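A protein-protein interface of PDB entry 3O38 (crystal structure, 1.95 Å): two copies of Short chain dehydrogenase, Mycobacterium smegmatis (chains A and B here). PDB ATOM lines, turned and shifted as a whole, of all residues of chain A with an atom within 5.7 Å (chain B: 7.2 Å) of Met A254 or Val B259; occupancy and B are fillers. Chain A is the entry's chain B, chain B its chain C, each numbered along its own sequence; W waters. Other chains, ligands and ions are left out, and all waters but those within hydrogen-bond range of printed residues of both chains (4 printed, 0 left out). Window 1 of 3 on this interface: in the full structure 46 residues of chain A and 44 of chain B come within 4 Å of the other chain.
Phe A245 touches its own counterpart, Phe B245. Met A254 touches Val B259, and with the chains exchanged Val A259 touches Met B254. 6 positions are printed for both chains. Of the 24 pairs that touch across the chains among the printed residues, 3 have their exchanged pair printed and touching as well.
Water W1 lies within hydrogen-bond range of the side-chain carboxylate of Glu A257 (2.7 Å) and the backbone carbonyl oxygen of Arg B265 (2.7 Å). Water W2 lies within hydrogen-bond range of N of Phe B230 (2.8 Å) and OH of Tyr A253 (3.0 Å). Water W3 bridges the backbone carbonyl oxygen of Gly A256 (2.8 Å) and the backbone carbonyl oxygen of Arg B265 (2.9 Å). Water W4 lies within hydrogen-bond range of O of Glu B238 (2.9 Å), N of Tyr A253 (3.1 Å), OG1 of Thr B242 (3.2 Å) and N of Ser A252 (3.4 Å).
Of the 22 printed residues of chain B, 13 touch a printed residue of chain A. Printed residues of chain B that touch a printed residue of chain A: Phe B230, Arg B232, Glu B238, Thr B242, Phe B245, Met B254, Val B259, Ser B260, Val B261, Ser B262, Ser B263, Gln B264 and Arg B265. Hydrophobic or aromatic side chains of chain B that line the printed part of chain A: Phe B230, Phe B245, Met B254, Val B259 and Val B261. Hydrophobic or aromatic side chains of chain A that line the printed part of chain B: Phe A245, Tyr A253, Met A254 and Val A259.
O of Ser A251 sits at hydrogen-bond distance from NH1 of Arg A198. The backbone NH (N) of Ile A199 lies within hydrogen-bond range of the side-chain hydroxyl (OG1) of Thr A255, 3.1 Å away. The backbone carbonyl oxygen of Met B254 is in hydrogen-bond range of the side-chain amide nitrogen of Asn B200 (3.1 Å). O of Ser B203 lies within hydrogen-bond range of N of Val B261 (2.8 Å). OE1 of Glu B238 lies within salt-bridge range of NH1 of Arg B232 (2.7 Å). N of Ser B263 lies within hydrogen-bond range of OG of Ser B260.
OG of Ser A252 is in hydrogen-bond range of OE2 of Glu B238 (2.7 Å). The backbone carbonyl oxygen (O) of Arg B232 is in hydrogen-bond range of the side-chain hydroxyl (OH) of Tyr A253, 2.8 Å away. N of Tyr A253 sits at hydrogen-bond distance from OE2 of Glu B238. The backbone NH of Thr A255 lies within hydrogen-bond range of the side-chain hydroxyl of Ser B262, at 3.1 Å. The backbone carbonyl oxygen (O) of Thr A255 lies within hydrogen-bond range of the side-chain amide nitrogen (NE2) of Gln B264 (2.9 Å). OG of Ser B262 is in hydrogen-bond range of OE2 of Glu A257, 2.6 Å away. The backbone NH (N) of Ser B263 is in hydrogen-bond range of the side-chain carboxylate (OE2) of Glu A257 (2.9 Å). The side-chain carboxylate (OE2) of Glu A257 sits at hydrogen-bond distance from the backbone NH (N) of Gln B264, at 2.7 Å. N of Arg B265 lies within hydrogen-bond range of OE1 of Glu A257 (3.0 Å).
Met A254 touches just these residues of chain B: Val B259, Ser B260, Val B261 and Ser B262. Printed residues of chain A within 4 Å of Ser B262: Tyr A253 (3.3 Å), Met A254 (3.5 Å), Thr A255 (3.1 Å) and Glu A257 (2.6 Å). Printed residues of chain A within 4 Å of Ser B263: Glu A257 (2.9 Å). Of the printed residues of chain A, Gln B264 touches Thr A255, Gly A256 and Glu A257.
Among the printed residues, pairs that only touch across the chains: Tyr A253 with Ser B262 (3.3 Å), Phe A245 with Phe B245 (3.3 Å), Gly A256 with Gln B264 (3.4 Å), Ser A252 with Phe B230 (3.4 Å), Glu A257 with Ser B260 (3.5 Å), Met A254 with Ser B262 (3.5 Å), Val A259 with Met B254 (3.5 Å), Met A254 with Val B259 (3.6 Å), Thr A255 with Phe B230 (3.7 Å), Tyr A253 with Phe B230 (3.7 Å), Phe A245 with Thr B242 (3.8 Å), Arg A198 with Phe B230 (3.8 Å), Met A254 with Ser B260 (3.9 Å), Tyr A253 with Val B261 (3.95 Å) and Met A254 with Val B261 (3.97 Å).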
ATOM      1  N   ARG A 198      -5.152  -8.634 -13.665  1.00  0.00           N
ATOM      2  CA  ARG A 198      -5.874  -9.644 -12.898  1.00  0.00           C
ATOM      3  C   ARG A 198      -7.272  -9.799 -13.494  1.00  0.00           C
ATOM      4  O   ARG A 198      -7.857  -8.818 -13.947  1.00  0.00           O
ATOM      5  CB  ARG A 198      -5.995  -9.234 -11.414  1.00  0.00           C
ATOM      6  CG  ARG A 198      -4.654  -8.960 -10.746  1.00  0.00           C
ATOM      7  CD  ARG A 198      -4.848  -8.777  -9.217  1.00  0.00           C
ATOM      8  NE  ARG A 198      -5.503  -7.510  -8.849  1.00  0.00           N
ATOM      9  CZ  ARG A 198      -6.754  -7.435  -8.412  1.00  0.00           C
ATOM     10  NH1 ARG A 198      -7.503  -8.543  -8.311  1.00  0.00           N
ATOM     11  NH2 ARG A 198      -7.258  -6.272  -8.053  1.00  0.00           N
ATOM     12  N   ILE A 199      -7.780 -11.029 -13.527  1.00  0.00           N
ATOM     13  CA  ILE A 199      -9.165 -11.325 -13.949  1.00  0.00           C
ATOM     14  C   ILE A 199      -9.910 -12.262 -12.966  1.00  0.00           C
ATOM     15  O   ILE A 199      -9.478 -13.408 -12.694  1.00  0.00           O
ATOM     16  CB  ILE A 199      -9.212 -11.968 -15.350  1.00  0.00           C
ATOM     17  CG1 ILE A 199      -8.329 -11.195 -16.375  1.00  0.00           C
ATOM     18  CG2 ILE A 199     -10.642 -12.108 -15.830  1.00  0.00           C
ATOM     19  CD1 ILE A 199      -8.231 -11.863 -17.736  1.00  0.00           C
ATOM     20  N   ASN A 200     -11.034 -11.788 -12.449  1.00  0.00           N
ATOM     21  CA  ASN A 200     -11.846 -12.600 -11.529  1.00  0.00           C
ATOM     22  C   ASN A 200     -13.297 -12.410 -11.911  1.00  0.00           C
ATOM     23  O   ASN A 200     -13.598 -11.592 -12.794  1.00  0.00           O
ATOM     24  CB  ASN A 200     -11.643 -12.211 -10.047  1.00  0.00           C
ATOM     25  CG  ASN A 200     -10.201 -12.383  -9.577  1.00  0.00           C
ATOM     26  OD1 ASN A 200      -9.782 -13.480  -9.194  1.00  0.00           O
ATOM     27  ND2 ASN A 200      -9.455 -11.289  -9.567  1.00  0.00           N
ATOM     28  N   PHE A 245     -14.708  -4.449  -4.992  1.00  0.00           N
ATOM     29  CA  PHE A 245     -13.605  -5.146  -4.285  1.00  0.00           C
ATOM     30  C   PHE A 245     -12.655  -5.848  -5.257  1.00  0.00           C
ATOM     31  O   PHE A 245     -11.443  -5.683  -5.175  1.00  0.00           O
ATOM     32  CB  PHE A 245     -14.152  -6.138  -3.223  1.00  0.00           C
ATOM     33  CG  PHE A 245     -13.192  -7.230  -2.834  1.00  0.00           C
ATOM     34  CD1 PHE A 245     -12.080  -6.957  -2.018  1.00  0.00           C
ATOM     35  CD2 PHE A 245     -13.409  -8.549  -3.266  1.00  0.00           C
ATOM     36  CE1 PHE A 245     -11.170  -7.997  -1.630  1.00  0.00           C
ATOM     37  CE2 PHE A 245     -12.536  -9.595  -2.904  1.00  0.00           C
ATOM     38  CZ  PHE A 245     -11.391  -9.327  -2.053  1.00  0.00           C
ATOM     39  N   LEU A 246     -13.212  -6.597  -6.195  1.00  0.00           N
ATOM     40  CA  LEU A 246     -12.402  -7.354  -7.145  1.00  0.00           C
ATOM     41  C   LEU A 246     -11.719  -6.448  -8.143  1.00  0.00           C
ATOM     42  O   LEU A 246     -10.732  -6.853  -8.734  1.00  0.00           O
ATOM     43  CB  LEU A 246     -13.281  -8.384  -7.907  1.00  0.00           C
ATOM     44  CG  LEU A 246     -13.819  -9.559  -7.091  1.00  0.00           C
ATOM     45  CD1 LEU A 246     -14.694 -10.405  -7.937  1.00  0.00           C
ATOM     46  CD2 LEU A 246     -12.616 -10.384  -6.563  1.00  0.00           C
ATOM     47  N   SER A 251      -8.216  -6.823  -3.393  1.00  0.00           N
ATOM     48  CA  SER A 251      -8.156  -8.201  -3.916  1.00  0.00           C
ATOM     49  C   SER A 251      -6.808  -8.443  -4.665  1.00  0.00           C
ATOM     50  O   SER A 251      -6.700  -9.338  -5.541  1.00  0.00           O
ATOM     51  CB  SER A 251      -9.368  -8.466  -4.825  1.00  0.00           C
ATOM     52  OG  SER A 251      -9.300  -7.565  -5.914  1.00  0.00           O
ATOM     53  N   SER A 252      -5.794  -7.640  -4.292  1.00  0.00           N
ATOM     54  CA  SER A 252      -4.435  -7.641  -4.872  1.00  0.00           C
ATOM     55  C   SER A 252      -3.877  -9.003  -5.322  1.00  0.00           C
ATOM     56  O   SER A 252      -3.330  -9.131  -6.422  1.00  0.00           O
ATOM     57  CB  SER A 252      -3.470  -7.067  -3.817  1.00  0.00           C
ATOM     58  OG  SER A 252      -2.183  -6.942  -4.346  1.00  0.00           O
ATOM     59  N   TYR A 253      -3.996 -10.010  -4.452  1.00  0.00           N
ATOM     60  CA  TYR A 253      -3.458 -11.359  -4.758  1.00  0.00           C
ATOM     61  C   TYR A 253      -4.378 -12.291  -5.559  1.00  0.00           C
ATOM     62  O   TYR A 253      -3.917 -13.302  -6.083  1.00  0.00           O
ATOM     63  CB  TYR A 253      -2.933 -12.040  -3.471  1.00  0.00           C
ATOM     64  CG  TYR A 253      -2.020 -13.213  -3.751  1.00  0.00           C
ATOM     65  CD1 TYR A 253      -0.722 -13.010  -4.253  1.00  0.00           C
ATOM     66  CD2 TYR A 253      -2.454 -14.527  -3.551  1.00  0.00           C
ATOM     67  CE1 TYR A 253       0.112 -14.098  -4.542  1.00  0.00           C
ATOM     68  CE2 TYR A 253      -1.611 -15.617  -3.832  1.00  0.00           C
ATOM     69  CZ  TYR A 253      -0.335 -15.390  -4.325  1.00  0.00           C
ATOM     70  OH  TYR A 253       0.511 -16.458  -4.624  1.00  0.00           O
ATOM     71  N   MET A 254      -5.660 -11.950  -5.675  1.00  0.00           N
ATOM     72  CA  MET A 254      -6.635 -12.799  -6.352  1.00  0.00           C
ATOM     73  C   MET A 254      -6.621 -12.672  -7.862  1.00  0.00           C
ATOM     74  O   MET A 254      -6.751 -11.579  -8.410  1.00  0.00           O
ATOM     75  CB  MET A 254      -8.066 -12.486  -5.866  1.00  0.00           C
ATOM     76  CG  MET A 254      -8.274 -12.766  -4.376  1.00  0.00           C
ATOM     77  SD  MET A 254      -9.924 -12.283  -3.824  1.00  0.00           S
ATOM     78  CE  MET A 254     -10.981 -13.370  -4.838  1.00  0.00           C
ATOM     79  N   THR A 255      -6.507 -13.809  -8.536  1.00  0.00           N
ATOM     80  CA  THR A 255      -6.764 -13.860  -9.973  1.00  0.00           C
ATOM     81  C   THR A 255      -7.363 -15.231 -10.298  1.00  0.00           C
ATOM     82  O   THR A 255      -7.096 -16.197  -9.572  1.00  0.00           O
ATOM     83  CB  THR A 255      -5.489 -13.572 -10.808  1.00  0.00           C
ATOM     84  OG1 THR A 255      -5.899 -13.107 -12.099  1.00  0.00           O
ATOM     85  CG2 THR A 255      -4.591 -14.841 -10.926  1.00  0.00           C
ATOM     86  N   GLY A 256      -8.208 -15.286 -11.336  1.00  0.00           N
ATOM     87  CA  GLY A 256      -8.851 -16.537 -11.771  1.00  0.00           C
ATOM     88  C   GLY A 256      -9.872 -17.093 -10.775  1.00  0.00           C
ATOM     89  O   GLY A 256     -10.157 -18.290 -10.799  1.00  0.00           O
ATOM     90  N   GLU A 257     -10.388 -16.237  -9.883  1.00  0.00           N
ATOM     91  CA  GLU A 257     -11.334 -16.649  -8.831  1.00  0.00           C
ATOM     92  C   GLU A 257     -12.750 -16.280  -9.192  1.00  0.00           C
ATOM     93  O   GLU A 257     -12.980 -15.364  -9.994  1.00  0.00           O
ATOM     94  CB  GLU A 257     -11.020 -16.014  -7.476  1.00  0.00           C
ATOM     95  CG  GLU A 257      -9.550 -16.158  -6.980  1.00  0.00           C
ATOM     96  CD  GLU A 257      -9.097 -17.612  -6.789  1.00  0.00           C
ATOM     97  OE1 GLU A 257      -9.946 -18.524  -6.830  1.00  0.00           O
ATOM     98  OE2 GLU A 257      -7.868 -17.823  -6.647  1.00  0.00           O
ATOM     99  N   VAL A 259     -16.351 -15.467  -7.126  1.00  0.00           N
ATOM    100  CA  VAL A 259     -16.858 -15.197  -5.787  1.00  0.00           C
ATOM    101  C   VAL A 259     -18.382 -15.297  -5.766  1.00  0.00           C
ATOM    102  O   VAL A 259     -19.082 -14.517  -6.429  1.00  0.00           O
ATOM    103  CB  VAL A 259     -16.399 -13.810  -5.312  1.00  0.00           C
ATOM    104  CG1 VAL A 259     -16.881 -13.538  -3.910  1.00  0.00           C
ATOM    105  CG2 VAL A 259     -14.861 -13.740  -5.355  1.00  0.00           C
ATOM    106  N   TRP B 165      -9.137 -28.199   0.263  1.00  0.00           N
ATOM    107  CA  TRP B 165      -9.504 -28.740  -1.035  1.00  0.00           C
ATOM    108  C   TRP B 165      -8.421 -29.600  -1.687  1.00  0.00           C
ATOM    109  O   TRP B 165      -8.714 -30.543  -2.440  1.00  0.00           O
ATOM    110  CB  TRP B 165      -9.795 -27.611  -2.029  1.00  0.00           C
ATOM    111  CG  TRP B 165     -10.895 -26.666  -1.675  1.00  0.00           C
ATOM    112  CD1 TRP B 165     -12.203 -26.969  -1.403  1.00  0.00           C
ATOM    113  CD2 TRP B 165     -10.787 -25.234  -1.621  1.00  0.00           C
ATOM    114  NE1 TRP B 165     -12.910 -25.799  -1.149  1.00  0.00           N
ATOM    115  CE2 TRP B 165     -12.059 -24.728  -1.267  1.00  0.00           C
ATOM    116  CE3 TRP B 165      -9.728 -24.339  -1.802  1.00  0.00           C
ATOM    117  CZ2 TRP B 165     -12.311 -23.375  -1.137  1.00  0.00           C
ATOM    118  CZ3 TRP B 165      -9.984 -22.964  -1.673  1.00  0.00           C
ATOM    119  CH2 TRP B 165     -11.260 -22.510  -1.342  1.00  0.00           C
ATOM    120  N   ASN B 200     -18.081 -15.608   6.999  1.00  0.00           N
ATOM    121  CA  ASN B 200     -17.375 -16.073   5.790  1.00  0.00           C
ATOM    122  C   ASN B 200     -15.937 -16.465   6.159  1.00  0.00           C
ATOM    123  O   ASN B 200     -15.507 -16.265   7.285  1.00  0.00           O
ATOM    124  CB  ASN B 200     -17.361 -15.019   4.673  1.00  0.00           C
ATOM    125  CG  ASN B 200     -18.767 -14.531   4.278  1.00  0.00           C
ATOM    126  OD1 ASN B 200     -19.458 -15.154   3.470  1.00  0.00           O
ATOM    127  ND2 ASN B 200     -19.174 -13.399   4.835  1.00  0.00           N
ATOM    128  N   ALA B 201     -15.213 -17.032   5.202  1.00  0.00           N
ATOM    129  CA  ALA B 201     -13.829 -17.420   5.403  1.00  0.00           C
ATOM    130  C   ALA B 201     -13.014 -16.955   4.231  1.00  0.00           C
ATOM    131  O   ALA B 201     -13.499 -16.893   3.075  1.00  0.00           O
ATOM    132  CB  ALA B 201     -13.697 -18.952   5.524  1.00  0.00           C
ATOM    133  N   VAL B 202     -11.761 -16.665   4.523  1.00  0.00           N
ATOM    134  CA  VAL B 202     -10.808 -16.529   3.460  1.00  0.00           C
ATOM    135  C   VAL B 202     -10.089 -17.875   3.409  1.00  0.00           C
ATOM    136  O   VAL B 202     -10.046 -18.586   4.413  1.00  0.00           O
ATOM    137  CB  VAL B 202      -9.838 -15.326   3.717  1.00  0.00           C
ATOM    138  CG1 VAL B 202      -8.910 -15.586   4.923  1.00  0.00           C
ATOM    139  CG2 VAL B 202      -9.036 -15.034   2.498  1.00  0.00           C
ATOM    140  N   SER B 203      -9.525 -18.209   2.250  1.00  0.00           N
ATOM    141  CA  SER B 203      -8.792 -19.469   2.057  1.00  0.00           C
ATOM    142  C   SER B 203      -7.426 -19.223   1.362  1.00  0.00           C
ATOM    143  O   SER B 203      -7.316 -19.229   0.144  1.00  0.00           O
ATOM    144  CB  SER B 203      -9.657 -20.482   1.286  1.00  0.00           C
ATOM    145  OG  SER B 203      -9.139 -21.786   1.440  1.00  0.00           O
ATOM    146  N   PRO B 204      -6.369 -19.011   2.153  1.00  0.00           N
ATOM    147  CA  PRO B 204      -5.033 -18.719   1.590  1.00  0.00           C
ATOM    148  C   PRO B 204      -4.416 -19.884   0.819  1.00  0.00           C
ATOM    149  O   PRO B 204      -4.536 -21.044   1.265  1.00  0.00           O
ATOM    150  CB  PRO B 204      -4.203 -18.371   2.850  1.00  0.00           C
ATOM    151  CG  PRO B 204      -5.254 -17.866   3.850  1.00  0.00           C
ATOM    152  CD  PRO B 204      -6.399 -18.823   3.614  1.00  0.00           C
ATOM    153  N   PHE B 230       1.029 -15.684 -10.153  1.00  0.00           N
ATOM    154  CA  PHE B 230       1.892 -14.503 -10.288  1.00  0.00           C
ATOM    155  C   PHE B 230       3.377 -14.861 -10.179  1.00  0.00           C
ATOM    156  O   PHE B 230       4.220 -13.997 -10.352  1.00  0.00           O
ATOM    157  CB  PHE B 230       1.619 -13.439  -9.228  1.00  0.00           C
ATOM    158  CG  PHE B 230       0.242 -12.829  -9.259  1.00  0.00           C
ATOM    159  CD1 PHE B 230      -0.614 -12.993 -10.344  1.00  0.00           C
ATOM    160  CD2 PHE B 230      -0.184 -12.047  -8.188  1.00  0.00           C
ATOM    161  CE1 PHE B 230      -1.904 -12.411 -10.338  1.00  0.00           C
ATOM    162  CE2 PHE B 230      -1.480 -11.455  -8.176  1.00  0.00           C
ATOM    163  CZ  PHE B 230      -2.327 -11.643  -9.277  1.00  0.00           C
ATOM    164  N   ARG B 232       4.817 -15.559  -7.384  1.00  0.00           N
ATOM    165  CA  ARG B 232       5.263 -15.086  -6.067  1.00  0.00           C
ATOM    166  C   ARG B 232       4.237 -15.541  -5.048  1.00  0.00           C
ATOM    167  O   ARG B 232       3.077 -15.795  -5.412  1.00  0.00           O
ATOM    168  CB  ARG B 232       5.425 -13.541  -6.045  1.00  0.00           C
ATOM    169  CG  ARG B 232       4.116 -12.764  -6.217  1.00  0.00           C
ATOM    170  CD  ARG B 232       4.200 -11.255  -5.962  1.00  0.00           C
ATOM    171  NE  ARG B 232       2.878 -10.600  -6.139  1.00  0.00           N
ATOM    172  CZ  ARG B 232       1.937 -10.468  -5.203  1.00  0.00           C
ATOM    173  NH1 ARG B 232       2.144 -10.904  -3.961  1.00  0.00           N
ATOM    174  NH2 ARG B 232       0.774  -9.865  -5.493  1.00  0.00           N
ATOM    175  N   GLU B 238      -1.781  -8.850   1.892  1.00  0.00           N
ATOM    176  CA  GLU B 238      -2.805  -9.135   0.868  1.00  0.00           C
ATOM    177  C   GLU B 238      -3.928 -10.026   1.401  1.00  0.00           C
ATOM    178  O   GLU B 238      -5.107  -9.788   1.101  1.00  0.00           O
ATOM    179  CB  GLU B 238      -2.179  -9.723  -0.401  1.00  0.00           C
ATOM    180  CG  GLU B 238      -1.256  -8.767  -1.143  1.00  0.00           C
ATOM    181  CD  GLU B 238      -0.548  -9.422  -2.315  1.00  0.00           C
ATOM    182  OE1 GLU B 238       0.359 -10.251  -2.084  1.00  0.00           O
ATOM    183  OE2 GLU B 238      -0.893  -9.112  -3.483  1.00  0.00           O
ATOM    184  N   THR B 242      -8.140  -8.917   2.090  1.00  0.00           N
ATOM    185  CA  THR B 242      -9.332  -9.705   1.771  1.00  0.00           C
ATOM    186  C   THR B 242     -10.168 -10.016   3.020  1.00  0.00           C
ATOM    187  O   THR B 242     -11.416 -10.049   2.980  1.00  0.00           O
ATOM    188  CB  THR B 242      -8.942 -10.981   1.002  1.00  0.00           C
ATOM    189  OG1 THR B 242      -8.346 -10.591  -0.250  1.00  0.00           O
ATOM    190  CG2 THR B 242     -10.163 -11.853   0.727  1.00  0.00           C
ATOM    191  N   PHE B 245     -12.192  -6.935   3.547  1.00  0.00           N
ATOM    192  CA  PHE B 245     -13.329  -6.956   2.646  1.00  0.00           C
ATOM    193  C   PHE B 245     -14.493  -7.735   3.230  1.00  0.00           C
ATOM    194  O   PHE B 245     -15.622  -7.251   3.237  1.00  0.00           O
ATOM    195  CB  PHE B 245     -12.927  -7.558   1.277  1.00  0.00           C
ATOM    196  CG  PHE B 245     -14.102  -8.003   0.462  1.00  0.00           C
ATOM    197  CD1 PHE B 245     -15.003  -7.059  -0.050  1.00  0.00           C
ATOM    198  CD2 PHE B 245     -14.334  -9.359   0.220  1.00  0.00           C
ATOM    199  CE1 PHE B 245     -16.114  -7.456  -0.775  1.00  0.00           C
ATOM    200  CE2 PHE B 245     -15.462  -9.751  -0.521  1.00  0.00           C
ATOM    201  CZ  PHE B 245     -16.333  -8.792  -1.016  1.00  0.00           C
ATOM    202  N   LEU B 246     -14.202  -8.948   3.687  1.00  0.00           N
ATOM    203  CA  LEU B 246     -15.191  -9.826   4.304  1.00  0.00           C
ATOM    204  C   LEU B 246     -15.727  -9.318   5.631  1.00  0.00           C
ATOM    205  O   LEU B 246     -16.834  -9.696   6.025  1.00  0.00           O
ATOM    206  CB  LEU B 246     -14.650 -11.249   4.471  1.00  0.00           C
ATOM    207  CG  LEU B 246     -14.435 -12.033   3.164  1.00  0.00           C
ATOM    208  CD1 LEU B 246     -13.871 -13.427   3.444  1.00  0.00           C
ATOM    209  CD2 LEU B 246     -15.725 -12.155   2.333  1.00  0.00           C
ATOM    210  N   MET B 254     -22.857 -11.300   1.344  1.00  0.00           N
ATOM    211  CA  MET B 254     -22.191 -12.560   1.464  1.00  0.00           C
ATOM    212  C   MET B 254     -22.264 -13.170   2.837  1.00  0.00           C
ATOM    213  O   MET B 254     -21.948 -12.553   3.771  1.00  0.00           O
ATOM    214  CB  MET B 254     -20.711 -12.454   1.069  1.00  0.00           C
ATOM    215  CG  MET B 254     -20.452 -11.994  -0.330  1.00  0.00           C
ATOM    216  SD  MET B 254     -18.746 -11.848  -0.806  1.00  0.00           S
ATOM    217  CE  MET B 254     -18.157 -13.482  -0.605  1.00  0.00           C
ATOM    218  N   GLU B 257     -19.693 -18.080   2.727  1.00  0.00           N
ATOM    219  CA  GLU B 257     -18.741 -18.231   1.604  1.00  0.00           C
ATOM    220  C   GLU B 257     -17.304 -18.447   2.068  1.00  0.00           C
ATOM    221  O   GLU B 257     -16.930 -18.110   3.214  1.00  0.00           O
ATOM    222  CB  GLU B 257     -18.773 -17.028   0.648  1.00  0.00           C
ATOM    223  CG  GLU B 257     -20.185 -16.531   0.259  1.00  0.00           C
ATOM    224  CD  GLU B 257     -20.992 -17.527  -0.588  1.00  0.00           C
ATOM    225  OE1 GLU B 257     -20.455 -18.552  -1.056  1.00  0.00           O
ATOM    226  OE2 GLU B 257     -22.214 -17.305  -0.751  1.00  0.00           O
ATOM    227  N   VAL B 258     -16.507 -18.973   1.129  1.00  0.00           N
ATOM    228  CA  VAL B 258     -15.095 -19.212   1.317  1.00  0.00           C
ATOM    229  C   VAL B 258     -14.380 -18.603   0.083  1.00  0.00           C
ATOM    230  O   VAL B 258     -14.658 -18.998  -1.043  1.00  0.00           O
ATOM    231  CB  VAL B 258     -14.808 -20.761   1.442  1.00  0.00           C
ATOM    232  CG1 VAL B 258     -13.340 -21.039   1.619  1.00  0.00           C
ATOM    233  CG2 VAL B 258     -15.578 -21.368   2.615  1.00  0.00           C
ATOM    234  N   VAL B 259     -13.509 -17.617   0.297  1.00  0.00           N
ATOM    235  CA  VAL B 259     -12.856 -16.905  -0.812  1.00  0.00           C
ATOM    236  C   VAL B 259     -11.412 -17.347  -0.932  1.00  0.00           C
ATOM    237  O   VAL B 259     -10.635 -17.153  -0.002  1.00  0.00           O
ATOM    238  CB  VAL B 259     -12.945 -15.365  -0.608  1.00  0.00           C
ATOM    239  CG1 VAL B 259     -12.166 -14.641  -1.723  1.00  0.00           C
ATOM    240  CG2 VAL B 259     -14.458 -14.909  -0.574  1.00  0.00           C
ATOM    241  N   SER B 260     -11.066 -17.971  -2.066  1.00  0.00           N
ATOM    242  CA  SER B 260      -9.708 -18.441  -2.312  1.00  0.00           C
ATOM    243  C   SER B 260      -8.747 -17.297  -2.599  1.00  0.00           C
ATOM    244  O   SER B 260      -9.013 -16.446  -3.434  1.00  0.00           O
ATOM    245  CB  SER B 260      -9.702 -19.431  -3.464  1.00  0.00           C
ATOM    246  OG  SER B 260      -8.399 -19.866  -3.773  1.00  0.00           O
ATOM    247  N   VAL B 261      -7.635 -17.268  -1.871  1.00  0.00           N
ATOM    248  CA  VAL B 261      -6.662 -16.207  -2.054  1.00  0.00           C
ATOM    249  C   VAL B 261      -5.265 -16.877  -2.074  1.00  0.00           C
ATOM    250  O   VAL B 261      -4.592 -16.891  -1.072  1.00  0.00           O
ATOM    251  CB  VAL B 261      -6.780 -15.121  -0.941  1.00  0.00           C
ATOM    252  CG1 VAL B 261      -5.787 -13.957  -1.183  1.00  0.00           C
ATOM    253  CG2 VAL B 261      -8.210 -14.570  -0.844  1.00  0.00           C
ATOM    254  N   SER B 262      -4.839 -17.448  -3.191  1.00  0.00           N
ATOM    255  CA  SER B 262      -5.570 -17.468  -4.484  1.00  0.00           C
ATOM    256  C   SER B 262      -5.134 -18.729  -5.197  1.00  0.00           C
ATOM    257  O   SER B 262      -3.956 -18.847  -5.612  1.00  0.00           O
ATOM    258  CB  SER B 262      -5.234 -16.220  -5.334  1.00  0.00           C
ATOM    259  OG  SER B 262      -5.825 -16.218  -6.655  1.00  0.00           O
ATOM    260  N   SER B 263      -6.072 -19.662  -5.364  1.00  0.00           N
ATOM    261  CA  SER B 263      -5.756 -20.948  -5.983  1.00  0.00           C
ATOM    262  C   SER B 263      -6.607 -21.248  -7.215  1.00  0.00           C
ATOM    263  O   SER B 263      -6.590 -22.371  -7.711  1.00  0.00           O
ATOM    264  CB  SER B 263      -5.876 -22.099  -4.976  1.00  0.00           C
ATOM    265  OG  SER B 263      -5.380 -21.735  -3.699  1.00  0.00           O
ATOM    266  N   GLN B 264      -7.327 -20.241  -7.724  1.00  0.00           N
ATOM    267  CA  GLN B 264      -8.250 -20.411  -8.903  1.00  0.00           C
ATOM    268  C   GLN B 264      -9.268 -21.524  -8.650  1.00  0.00           C
ATOM    269  O   GLN B 264      -9.432 -22.437  -9.472  1.00  0.00           O
ATOM    270  CB  GLN B 264      -7.521 -20.644 -10.246  1.00  0.00           C
ATOM    271  CG  GLN B 264      -6.608 -19.522 -10.684  1.00  0.00           C
ATOM    272  CD  GLN B 264      -5.333 -19.450  -9.836  1.00  0.00           C
ATOM    273  OE1 GLN B 264      -4.584 -20.414  -9.770  1.00  0.00           O
ATOM    274  NE2 GLN B 264      -5.083 -18.308  -9.210  1.00  0.00           N
ATOM    275  N   ARG B 265      -9.896 -21.447  -7.477  1.00  0.00           N
ATOM    276  CA  ARG B 265     -10.816 -22.455  -7.005  1.00  0.00           C
ATOM    277  C   ARG B 265     -12.084 -22.421  -7.890  1.00  0.00           C
ATOM    278  O   ARG B 265     -12.748 -21.384  -7.995  1.00  0.00           O
ATOM    279  CB  ARG B 265     -11.130 -22.211  -5.526  1.00  0.00           C
ATOM    280  CG  ARG B 265     -12.313 -22.987  -5.005  1.00  0.00           C
ATOM    281  CD  ARG B 265     -11.995 -24.504  -4.880  1.00  0.00           C
ATOM    282  NE  ARG B 265     -13.217 -25.252  -4.533  1.00  0.00           N
ATOM    283  CZ  ARG B 265     -13.418 -26.554  -4.768  1.00  0.00           C
ATOM    284  NH1 ARG B 265     -12.489 -27.294  -5.350  1.00  0.00           N
ATOM    285  NH2 ARG B 265     -14.571 -27.119  -4.435  1.00  0.00           N
HETATM  286  O   HOH W   1     -12.577 -18.972  -6.826  1.00  0.00           O
HETATM  287  O   HOH W   2       0.208 -15.888  -7.532  1.00  0.00           O
HETATM  288  O   HOH W   3     -12.281 -20.066 -10.555  1.00  0.00           O
HETATM  289  O   HOH W   4      -5.641  -9.883  -1.783  1.00  0.00           O
